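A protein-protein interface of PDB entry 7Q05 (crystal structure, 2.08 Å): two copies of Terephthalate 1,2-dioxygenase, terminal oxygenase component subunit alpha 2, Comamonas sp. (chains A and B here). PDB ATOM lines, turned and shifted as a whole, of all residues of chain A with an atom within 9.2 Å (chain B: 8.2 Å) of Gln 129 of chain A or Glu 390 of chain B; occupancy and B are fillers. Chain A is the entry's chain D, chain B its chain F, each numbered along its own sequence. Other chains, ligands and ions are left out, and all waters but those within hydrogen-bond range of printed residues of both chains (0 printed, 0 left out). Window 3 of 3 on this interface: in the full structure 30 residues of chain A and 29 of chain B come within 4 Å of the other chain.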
ATOM      1  N   PHE A 122      11.160  31.089  27.439  1.00  0.00           N
ATOM      2  CA  PHE A 122      12.530  30.858  26.947  1.00  0.00           C
ATOM      3  C   PHE A 122      12.654  31.418  25.526  1.00  0.00           C
ATOM      4  O   PHE A 122      13.431  30.854  24.720  1.00  0.00           O
ATOM      5  CB  PHE A 122      12.827  29.357  26.998  1.00  0.00           C
ATOM      6  CG  PHE A 122      12.657  28.702  28.347  1.00  0.00           C
ATOM      7  CD1 PHE A 122      12.882  29.393  29.529  1.00  0.00           C
ATOM      8  CD2 PHE A 122      12.356  27.356  28.421  1.00  0.00           C
ATOM      9  CE1 PHE A 122      12.756  28.757  30.753  1.00  0.00           C
ATOM     10  CE2 PHE A 122      12.226  26.719  29.648  1.00  0.00           C
ATOM     11  CZ  PHE A 122      12.412  27.426  30.812  1.00  0.00           C
ATOM     12  N   GLU A 123      11.922  32.497  25.232  1.00  0.00           N
ATOM     13  CA  GLU A 123      12.024  33.223  23.932  1.00  0.00           C
ATOM     14  C   GLU A 123      13.488  33.517  23.606  1.00  0.00           C
ATOM     15  O   GLU A 123      13.853  33.332  22.452  1.00  0.00           O
ATOM     16  CB  GLU A 123      11.239  34.541  23.924  1.00  0.00           C
ATOM     17  CG  GLU A 123      11.229  35.189  22.545  1.00  0.00           C
ATOM     18  CD  GLU A 123      10.472  36.502  22.422  1.00  0.00           C
ATOM     19  OE1 GLU A 123       9.611  36.817  23.298  1.00  0.00           O
ATOM     20  OE2 GLU A 123      10.676  37.151  21.396  1.00  0.00           O
ATOM     21  N   LYS A 124      14.284  33.974  24.578  1.00  0.00           N
ATOM     22  CA  LYS A 124      15.673  34.467  24.341  1.00  0.00           C
ATOM     23  C   LYS A 124      16.664  33.370  24.717  1.00  0.00           C
ATOM     24  O   LYS A 124      17.769  33.655  24.993  1.00  0.00           O
ATOM     25  CB  LYS A 124      15.959  35.730  25.166  1.00  0.00           C
ATOM     26  CG  LYS A 124      14.897  36.838  25.145  1.00  0.00           C
ATOM     27  CD  LYS A 124      14.970  37.796  23.963  1.00  0.00           C
ATOM     28  CE  LYS A 124      14.853  37.106  22.618  1.00  0.00           C
ATOM     29  NZ  LYS A 124      14.123  37.929  21.625  1.00  0.00           N
ATOM     30  N   GLY A 125      16.238  32.132  24.755  1.00  0.00           N
ATOM     31  CA  GLY A 125      17.114  31.012  25.148  1.00  0.00           C
ATOM     32  C   GLY A 125      17.295  30.933  26.651  1.00  0.00           C
ATOM     33  O   GLY A 125      16.695  31.733  27.411  1.00  0.00           O
ATOM     34  N   VAL A 126      18.061  29.924  27.064  1.00  0.00           N
ATOM     35  CA  VAL A 126      18.369  29.630  28.490  1.00  0.00           C
ATOM     36  C   VAL A 126      19.882  29.539  28.561  1.00  0.00           C
ATOM     37  O   VAL A 126      20.468  28.804  27.740  1.00  0.00           O
ATOM     38  CB  VAL A 126      17.713  28.327  28.969  1.00  0.00           C
ATOM     39  CG1 VAL A 126      18.288  27.882  30.308  1.00  0.00           C
ATOM     40  CG2 VAL A 126      16.195  28.465  29.027  1.00  0.00           C
ATOM     41  N   LYS A 127      20.482  30.342  29.430  1.00  0.00           N
ATOM     42  CA  LYS A 127      21.952  30.533  29.436  1.00  0.00           C
ATOM     43  C   LYS A 127      22.327  31.027  28.033  1.00  0.00           C
ATOM     44  O   LYS A 127      21.665  31.976  27.551  1.00  0.00           O
ATOM     45  CB  LYS A 127      22.645  29.233  29.878  1.00  0.00           C
ATOM     46  CG  LYS A 127      23.083  29.148  31.345  1.00  0.00           C
ATOM     47  CD  LYS A 127      22.057  28.626  32.384  1.00  0.00           C
ATOM     48  CE  LYS A 127      21.544  27.230  32.107  1.00  0.00           C
ATOM     49  NZ  LYS A 127      22.654  26.247  32.120  1.00  0.00           N
ATOM     50  N   GLY A 128      23.278  30.381  27.357  1.00  0.00           N
ATOM     51  CA  GLY A 128      23.757  30.826  26.033  1.00  0.00           C
ATOM     52  C   GLY A 128      22.752  30.571  24.905  1.00  0.00           C
ATOM     53  O   GLY A 128      22.883  31.236  23.862  1.00  0.00           O
ATOM     54  N   GLN A 129      21.791  29.658  25.066  1.00  0.00           N
ATOM     55  CA  GLN A 129      21.506  28.709  23.963  1.00  0.00           C
ATOM     56  C   GLN A 129      20.003  28.472  23.780  1.00  0.00           C
ATOM     57  O   GLN A 129      19.202  28.734  24.692  1.00  0.00           O
ATOM     58  CB  GLN A 129      22.318  27.439  24.220  1.00  0.00           C
ATOM     59  CG  GLN A 129      22.476  27.099  25.701  1.00  0.00           C
ATOM     60  CD  GLN A 129      23.586  26.106  25.927  1.00  0.00           C
ATOM     61  OE1 GLN A 129      24.629  26.196  25.291  1.00  0.00           O
ATOM     62  NE2 GLN A 129      23.352  25.161  26.830  1.00  0.00           N
ATOM     63  N   GLY A 130      19.647  28.049  22.563  1.00  0.00           N
ATOM     64  CA  GLY A 130      18.259  27.823  22.114  1.00  0.00           C
ATOM     65  C   GLY A 130      17.455  29.119  22.064  1.00  0.00           C
ATOM     66  O   GLY A 130      18.040  30.225  21.923  1.00  0.00           O
ATOM     67  N   GLY A 131      16.132  29.003  22.223  1.00  0.00           N
ATOM     68  CA  GLY A 131      15.166  30.124  22.063  1.00  0.00           C
ATOM     69  C   GLY A 131      14.849  30.303  20.562  1.00  0.00           C
ATOM     70  O   GLY A 131      15.258  29.451  19.690  1.00  0.00           O
ATOM     71  N   MET A 132      14.064  31.411  20.315  1.00  0.00           N
ATOM     72  CA  MET A 132      13.638  31.812  18.931  1.00  0.00           C
ATOM     73  C   MET A 132      14.781  32.451  18.132  1.00  0.00           C
ATOM     74  O   MET A 132      15.720  33.008  18.690  1.00  0.00           O
ATOM     75  CB  MET A 132      12.448  32.762  19.048  1.00  0.00           C
ATOM     76  CG  MET A 132      11.272  32.094  19.697  1.00  0.00           C
ATOM     77  SD  MET A 132      10.854  30.554  18.811  1.00  0.00           S
ATOM     78  CE  MET A 132       9.141  30.275  19.262  1.00  0.00           C
ATOM     79  N   LYS B 231      23.186  20.495  33.672  1.00  0.00           N
ATOM     80  CA  LYS B 231      23.233  20.713  32.214  1.00  0.00           C
ATOM     81  C   LYS B 231      22.496  19.535  31.561  1.00  0.00           C
ATOM     82  O   LYS B 231      22.401  18.454  32.145  1.00  0.00           O
ATOM     83  CB  LYS B 231      24.683  21.029  31.805  1.00  0.00           C
ATOM     84  CG  LYS B 231      25.547  19.911  31.226  1.00  0.00           C
ATOM     85  CD  LYS B 231      25.774  20.031  29.695  1.00  0.00           C
ATOM     86  CE  LYS B 231      25.826  18.708  28.944  1.00  0.00           C
ATOM     87  NZ  LYS B 231      27.034  17.919  29.292  1.00  0.00           N
ATOM     88  N   GLY B 232      21.887  19.809  30.423  1.00  0.00           N
ATOM     89  CA  GLY B 232      21.213  18.817  29.586  1.00  0.00           C
ATOM     90  C   GLY B 232      21.480  19.077  28.119  1.00  0.00           C
ATOM     91  O   GLY B 232      22.136  20.082  27.781  1.00  0.00           O
ATOM     92  N   GLY B 233      20.984  18.198  27.268  1.00  0.00           N
ATOM     93  CA  GLY B 233      21.154  18.337  25.822  1.00  0.00           C
ATOM     94  C   GLY B 233      20.180  17.459  25.094  1.00  0.00           C
ATOM     95  O   GLY B 233      19.465  16.661  25.755  1.00  0.00           O
ATOM     96  N   VAL B 234      20.184  17.619  23.788  1.00  0.00           N
ATOM     97  CA  VAL B 234      19.339  16.867  22.847  1.00  0.00           C
ATOM     98  C   VAL B 234      20.269  16.281  21.800  1.00  0.00           C
ATOM     99  O   VAL B 234      21.077  16.997  21.292  1.00  0.00           O
ATOM    100  CB  VAL B 234      18.276  17.786  22.233  1.00  0.00           C
ATOM    101  CG1 VAL B 234      17.409  17.027  21.257  1.00  0.00           C
ATOM    102  CG2 VAL B 234      17.456  18.468  23.303  1.00  0.00           C
ATOM    103  N   ILE B 235      20.149  14.999  21.536  1.00  0.00           N
ATOM    104  CA  ILE B 235      20.869  14.323  20.442  1.00  0.00           C
ATOM    105  C   ILE B 235      19.829  13.914  19.418  1.00  0.00           C
ATOM    106  O   ILE B 235      18.773  13.394  19.811  1.00  0.00           O
ATOM    107  CB  ILE B 235      21.628  13.117  20.992  1.00  0.00           C
ATOM    108  CG1 ILE B 235      22.757  13.577  21.909  1.00  0.00           C
ATOM    109  CG2 ILE B 235      22.138  12.253  19.845  1.00  0.00           C
ATOM    110  CD1 ILE B 235      23.272  12.455  22.792  1.00  0.00           C
ATOM    111  N   TYR B 246      18.612  14.429  27.597  1.00  0.00           N
ATOM    112  CA  TYR B 246      19.327  13.981  28.806  1.00  0.00           C
ATOM    113  C   TYR B 246      19.575  15.171  29.730  1.00  0.00           C
ATOM    114  O   TYR B 246      19.578  16.343  29.283  1.00  0.00           O
ATOM    115  CB  TYR B 246      20.606  13.239  28.432  1.00  0.00           C
ATOM    116  CG  TYR B 246      21.668  14.113  27.847  1.00  0.00           C
ATOM    117  CD1 TYR B 246      21.720  14.384  26.493  1.00  0.00           C
ATOM    118  CD2 TYR B 246      22.613  14.713  28.661  1.00  0.00           C
ATOM    119  CE1 TYR B 246      22.685  15.232  25.958  1.00  0.00           C
ATOM    120  CE2 TYR B 246      23.568  15.573  28.144  1.00  0.00           C
ATOM    121  CZ  TYR B 246      23.613  15.833  26.788  1.00  0.00           C
ATOM    122  OH  TYR B 246      24.582  16.673  26.301  1.00  0.00           O
ATOM    123  N   MET B 248      22.054  15.900  33.548  1.00  0.00           N
ATOM    124  CA  MET B 248      23.181  15.356  34.361  1.00  0.00           C
ATOM    125  C   MET B 248      23.735  16.443  35.284  1.00  0.00           C
ATOM    126  O   MET B 248      23.675  17.648  34.918  1.00  0.00           O
ATOM    127  CB  MET B 248      24.306  14.847  33.451  1.00  0.00           C
ATOM    128  CG  MET B 248      24.829  15.909  32.449  1.00  0.00           C
ATOM    129  SD  MET B 248      25.952  15.297  31.141  1.00  0.00           S
ATOM    130  CE  MET B 248      27.261  14.559  32.126  1.00  0.00           C
ATOM    131  N   MET B 381      11.969  27.092  17.639  1.00  0.00           N
ATOM    132  CA  MET B 381      12.833  27.159  18.836  1.00  0.00           C
ATOM    133  C   MET B 381      14.143  26.396  18.543  1.00  0.00           C
ATOM    134  O   MET B 381      14.085  25.222  18.130  1.00  0.00           O
ATOM    135  CB  MET B 381      12.010  26.534  19.964  1.00  0.00           C
ATOM    136  CG  MET B 381      12.217  27.089  21.295  1.00  0.00           C
ATOM    137  SD  MET B 381      11.671  28.774  21.529  1.00  0.00           S
ATOM    138  CE  MET B 381      12.080  28.694  23.266  1.00  0.00           C
ATOM    139  N   GLY B 382      15.299  27.051  18.703  1.00  0.00           N
ATOM    140  CA  GLY B 382      16.620  26.492  18.345  1.00  0.00           C
ATOM    141  C   GLY B 382      16.907  26.538  16.843  1.00  0.00           C
ATOM    142  O   GLY B 382      17.749  25.744  16.410  1.00  0.00           O
ATOM    143  N   GLY B 387      19.552  18.823  14.183  1.00  0.00           N
ATOM    144  CA  GLY B 387      20.751  18.195  14.769  1.00  0.00           C
ATOM    145  C   GLY B 387      20.826  18.372  16.275  1.00  0.00           C
ATOM    146  O   GLY B 387      19.957  19.032  16.866  1.00  0.00           O
ATOM    147  N   SER B 388      21.841  17.770  16.879  1.00  0.00           N
ATOM    148  CA  SER B 388      22.102  17.793  18.336  1.00  0.00           C
ATOM    149  C   SER B 388      22.346  19.220  18.827  1.00  0.00           C
ATOM    150  O   SER B 388      22.779  20.051  18.046  1.00  0.00           O
ATOM    151  CB  SER B 388      23.225  16.862  18.651  1.00  0.00           C
ATOM    152  OG  SER B 388      22.848  15.581  18.174  1.00  0.00           O
ATOM    153  N   SER B 389      22.063  19.457  20.104  1.00  0.00           N
ATOM    154  CA  SER B 389      22.189  20.760  20.798  1.00  0.00           C
ATOM    155  C   SER B 389      22.634  20.526  22.240  1.00  0.00           C
ATOM    156  O   SER B 389      22.174  19.562  22.854  1.00  0.00           O
ATOM    157  CB  SER B 389      20.872  21.481  20.790  1.00  0.00           C
ATOM    158  OG  SER B 389      20.656  22.104  19.547  1.00  0.00           O
ATOM    159  N   GLU B 390      23.464  21.416  22.755  1.00  0.00           N
ATOM    160  CA  GLU B 390      23.596  21.683  24.210  1.00  0.00           C
ATOM    161  C   GLU B 390      22.344  22.475  24.614  1.00  0.00           C
ATOM    162  O   GLU B 390      21.856  23.296  23.802  1.00  0.00           O
ATOM    163  CB  GLU B 390      24.893  22.440  24.530  1.00  0.00           C
ATOM    164  CG  GLU B 390      26.173  21.812  23.997  1.00  0.00           C
ATOM    165  CD  GLU B 390      26.512  20.454  24.588  1.00  0.00           C
ATOM    166  OE1 GLU B 390      25.841  19.459  24.226  1.00  0.00           O
ATOM    167  OE2 GLU B 390      27.429  20.392  25.422  1.00  0.00           O
ATOM    168  N   GLY B 391      21.795  22.178  25.787  1.00  0.00           N
ATOM    169  CA  GLY B 391      20.543  22.782  26.264  1.00  0.00           C
ATOM    170  C   GLY B 391      19.341  22.089  25.651  1.00  0.00           C
ATOM    171  O   GLY B 391      19.508  21.292  24.688  1.00  0.00           O
ATOM    172  N   ARG B 392      18.167  22.409  26.189  1.00  0.00           N
ATOM    173  CA  ARG B 392      16.888  21.750  25.855  1.00  0.00           C
ATOM    174  C   ARG B 392      15.790  22.756  25.498  1.00  0.00           C
ATOM    175  O   ARG B 392      14.730  22.297  25.119  1.00  0.00           O
ATOM    176  CB  ARG B 392      16.552  20.866  27.061  1.00  0.00           C
ATOM    177  CG  ARG B 392      17.403  19.606  27.104  1.00  0.00           C
ATOM    178  CD  ARG B 392      17.923  19.274  28.484  1.00  0.00           C
ATOM    179  NE  ARG B 392      16.870  19.018  29.461  1.00  0.00           N
ATOM    180  CZ  ARG B 392      16.854  19.485  30.713  1.00  0.00           C
ATOM    181  NH1 ARG B 392      15.864  19.160  31.526  1.00  0.00           N
ATOM    182  NH2 ARG B 392      17.795  20.317  31.129  1.00  0.00           N
ATOM    183  N   ALA B 393      16.061  24.062  25.528  1.00  0.00           N
ATOM    184  CA  ALA B 393      15.173  25.156  25.041  1.00  0.00           C
ATOM    185  C   ALA B 393      15.273  25.243  23.506  1.00  0.00           C
ATOM    186  O   ALA B 393      15.566  26.314  22.943  1.00  0.00           O
ATOM    187  CB  ALA B 393      15.531  26.441  25.738  1.00  0.00           C
ATOM    188  N   THR B 394      14.949  24.128  22.849  1.00  0.00           N
ATOM    189  CA  THR B 394      14.999  23.929  21.384  1.00  0.00           C
ATOM    190  C   THR B 394      13.873  22.981  20.991  1.00  0.00           C
ATOM    191  O   THR B 394      13.427  22.235  21.865  1.00  0.00           O
ATOM    192  CB  THR B 394      16.360  23.345  20.993  1.00  0.00           C
ATOM    193  OG1 THR B 394      16.350  23.121  19.581  1.00  0.00           O
ATOM    194  CG2 THR B 394      16.674  22.047  21.713  1.00  0.00           C
ATOM    195  N   THR B 396      14.572  21.069  18.110  1.00  0.00           N
ATOM    196  CA  THR B 396      15.398  20.393  17.078  1.00  0.00           C
ATOM    197  C   THR B 396      14.953  18.936  16.905  1.00  0.00           C
ATOM    198  O   THR B 396      14.842  18.510  15.738  1.00  0.00           O
ATOM    199  CB  THR B 396      16.897  20.525  17.367  1.00  0.00           C
ATOM    200  OG1 THR B 396      17.557  19.958  16.242  1.00  0.00           O
ATOM    201  CG2 THR B 396      17.328  19.835  18.641  1.00  0.00           C
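Of the printed residues of chain B, Phe 122 of chain A touches Met 381 (2.9 Å).
No residue of chain B comes within 4 Å of Gly 128 of chain A.
Of chain B, only Glu 390 and Gly 391 come within 4 Å of Gln 129 of chain A.
Gly 130 of chain A touches just one residue of chain B: Ala 393 (3.2 Å).
Of the printed residues of chain B, Met 132 of chain A touches Met 381.
Of the printed residues of chain A, Met 381 of chain B touches Phe 122 (2.9 Å), Gly 131 (3.4 Å) and Met 132 (3.4 Å).
Of the printed residues of chain A, Gly 382 of chain B touches Gly 131.
Ser 389 of chain B touches none of the printed residues of chain A.
Of chain A, only Gln 129 (3.6 Å) comes within 4 Å of Glu 390 of chain B.
Of the printed residues of chain A, Ala 393 of chain B touches Val 126 (3.9 Å), Gly 130 (3.2 Å) and Gly 131 (2.8 Å).
The nearest residue of chain B that does not touch Gln 129 of chain A is Ala 393 of chain B (4.5 Å).
The nearest residue of chain A that does not touch Glu 390 of chain B is Gly 130 of chain A (5.4 Å).
The nearest printed residue of chain A that does not touch Met 381 of chain B is Glu 123 of chain A (4.3 Å).
The backbone carbonyl oxygen (O) of Glu 123 of chain A is in hydrogen-bond range of the backbone NH (N) of Met 132 of chain A (2.9 Å).
O of Gly 232 of chain B lies within hydrogen-bond range of N of Gly 391 of chain B (2.9 Å).
The side-chain hydroxyl (OG1) of Thr 394 of chain B sits at hydrogen-bond distance from the backbone carbonyl oxygen (O) of Met 381 of chain B, 3.4 Å away.
O of Phe 122 of chain A touches CE of Met 381 of chain B, at 2.9 Å.
Val 126 of chain A touches Ala 393 of chain B.
NE2 of Gln 129 of chain A touches C of Glu 390 of chain B (3.6 Å).
NE2 of Gln 129 of chain A touches N of Gly 391 of chain B (3.5 Å).
Gly 130 of chain A touches Ala 393 of chain B (CA to O, 3.2 Å).
O of Gly 131 of chain A touches CA of Met 381 of chain B (3.4 Å).
Of the 11 printed residues of chain A, 6 touch a printed residue of chain B.
Hydrophobic or aromatic side chains of chain A within 4 Å of the printed part of chain B: Phe 122, Val 126 and Met 132.
Among the printed residues, no Asp or Glu carboxylate lies within 4 Å of a Lys or Arg side-chain nitrogen of the other chain.
No position is printed for both chains.
Of the 9 pairs that touch across the chains among the printed residues, none has its exchanged pair printed and touching as well.
O of Gly 131 of chain A lies within hydrogen-bond range of N of Gly 382 of chain B (2.6 Å).
The backbone NH of Gly 131 of chain A sits at hydrogen-bond distance from the backbone carbonyl oxygen of Ala 393 of chain B (2.8 Å).
The side-chain sulfur (SD) of Met 381 of chain B sits close to the backbone NH (N) of Met 132 of chain A (3.8 Å).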
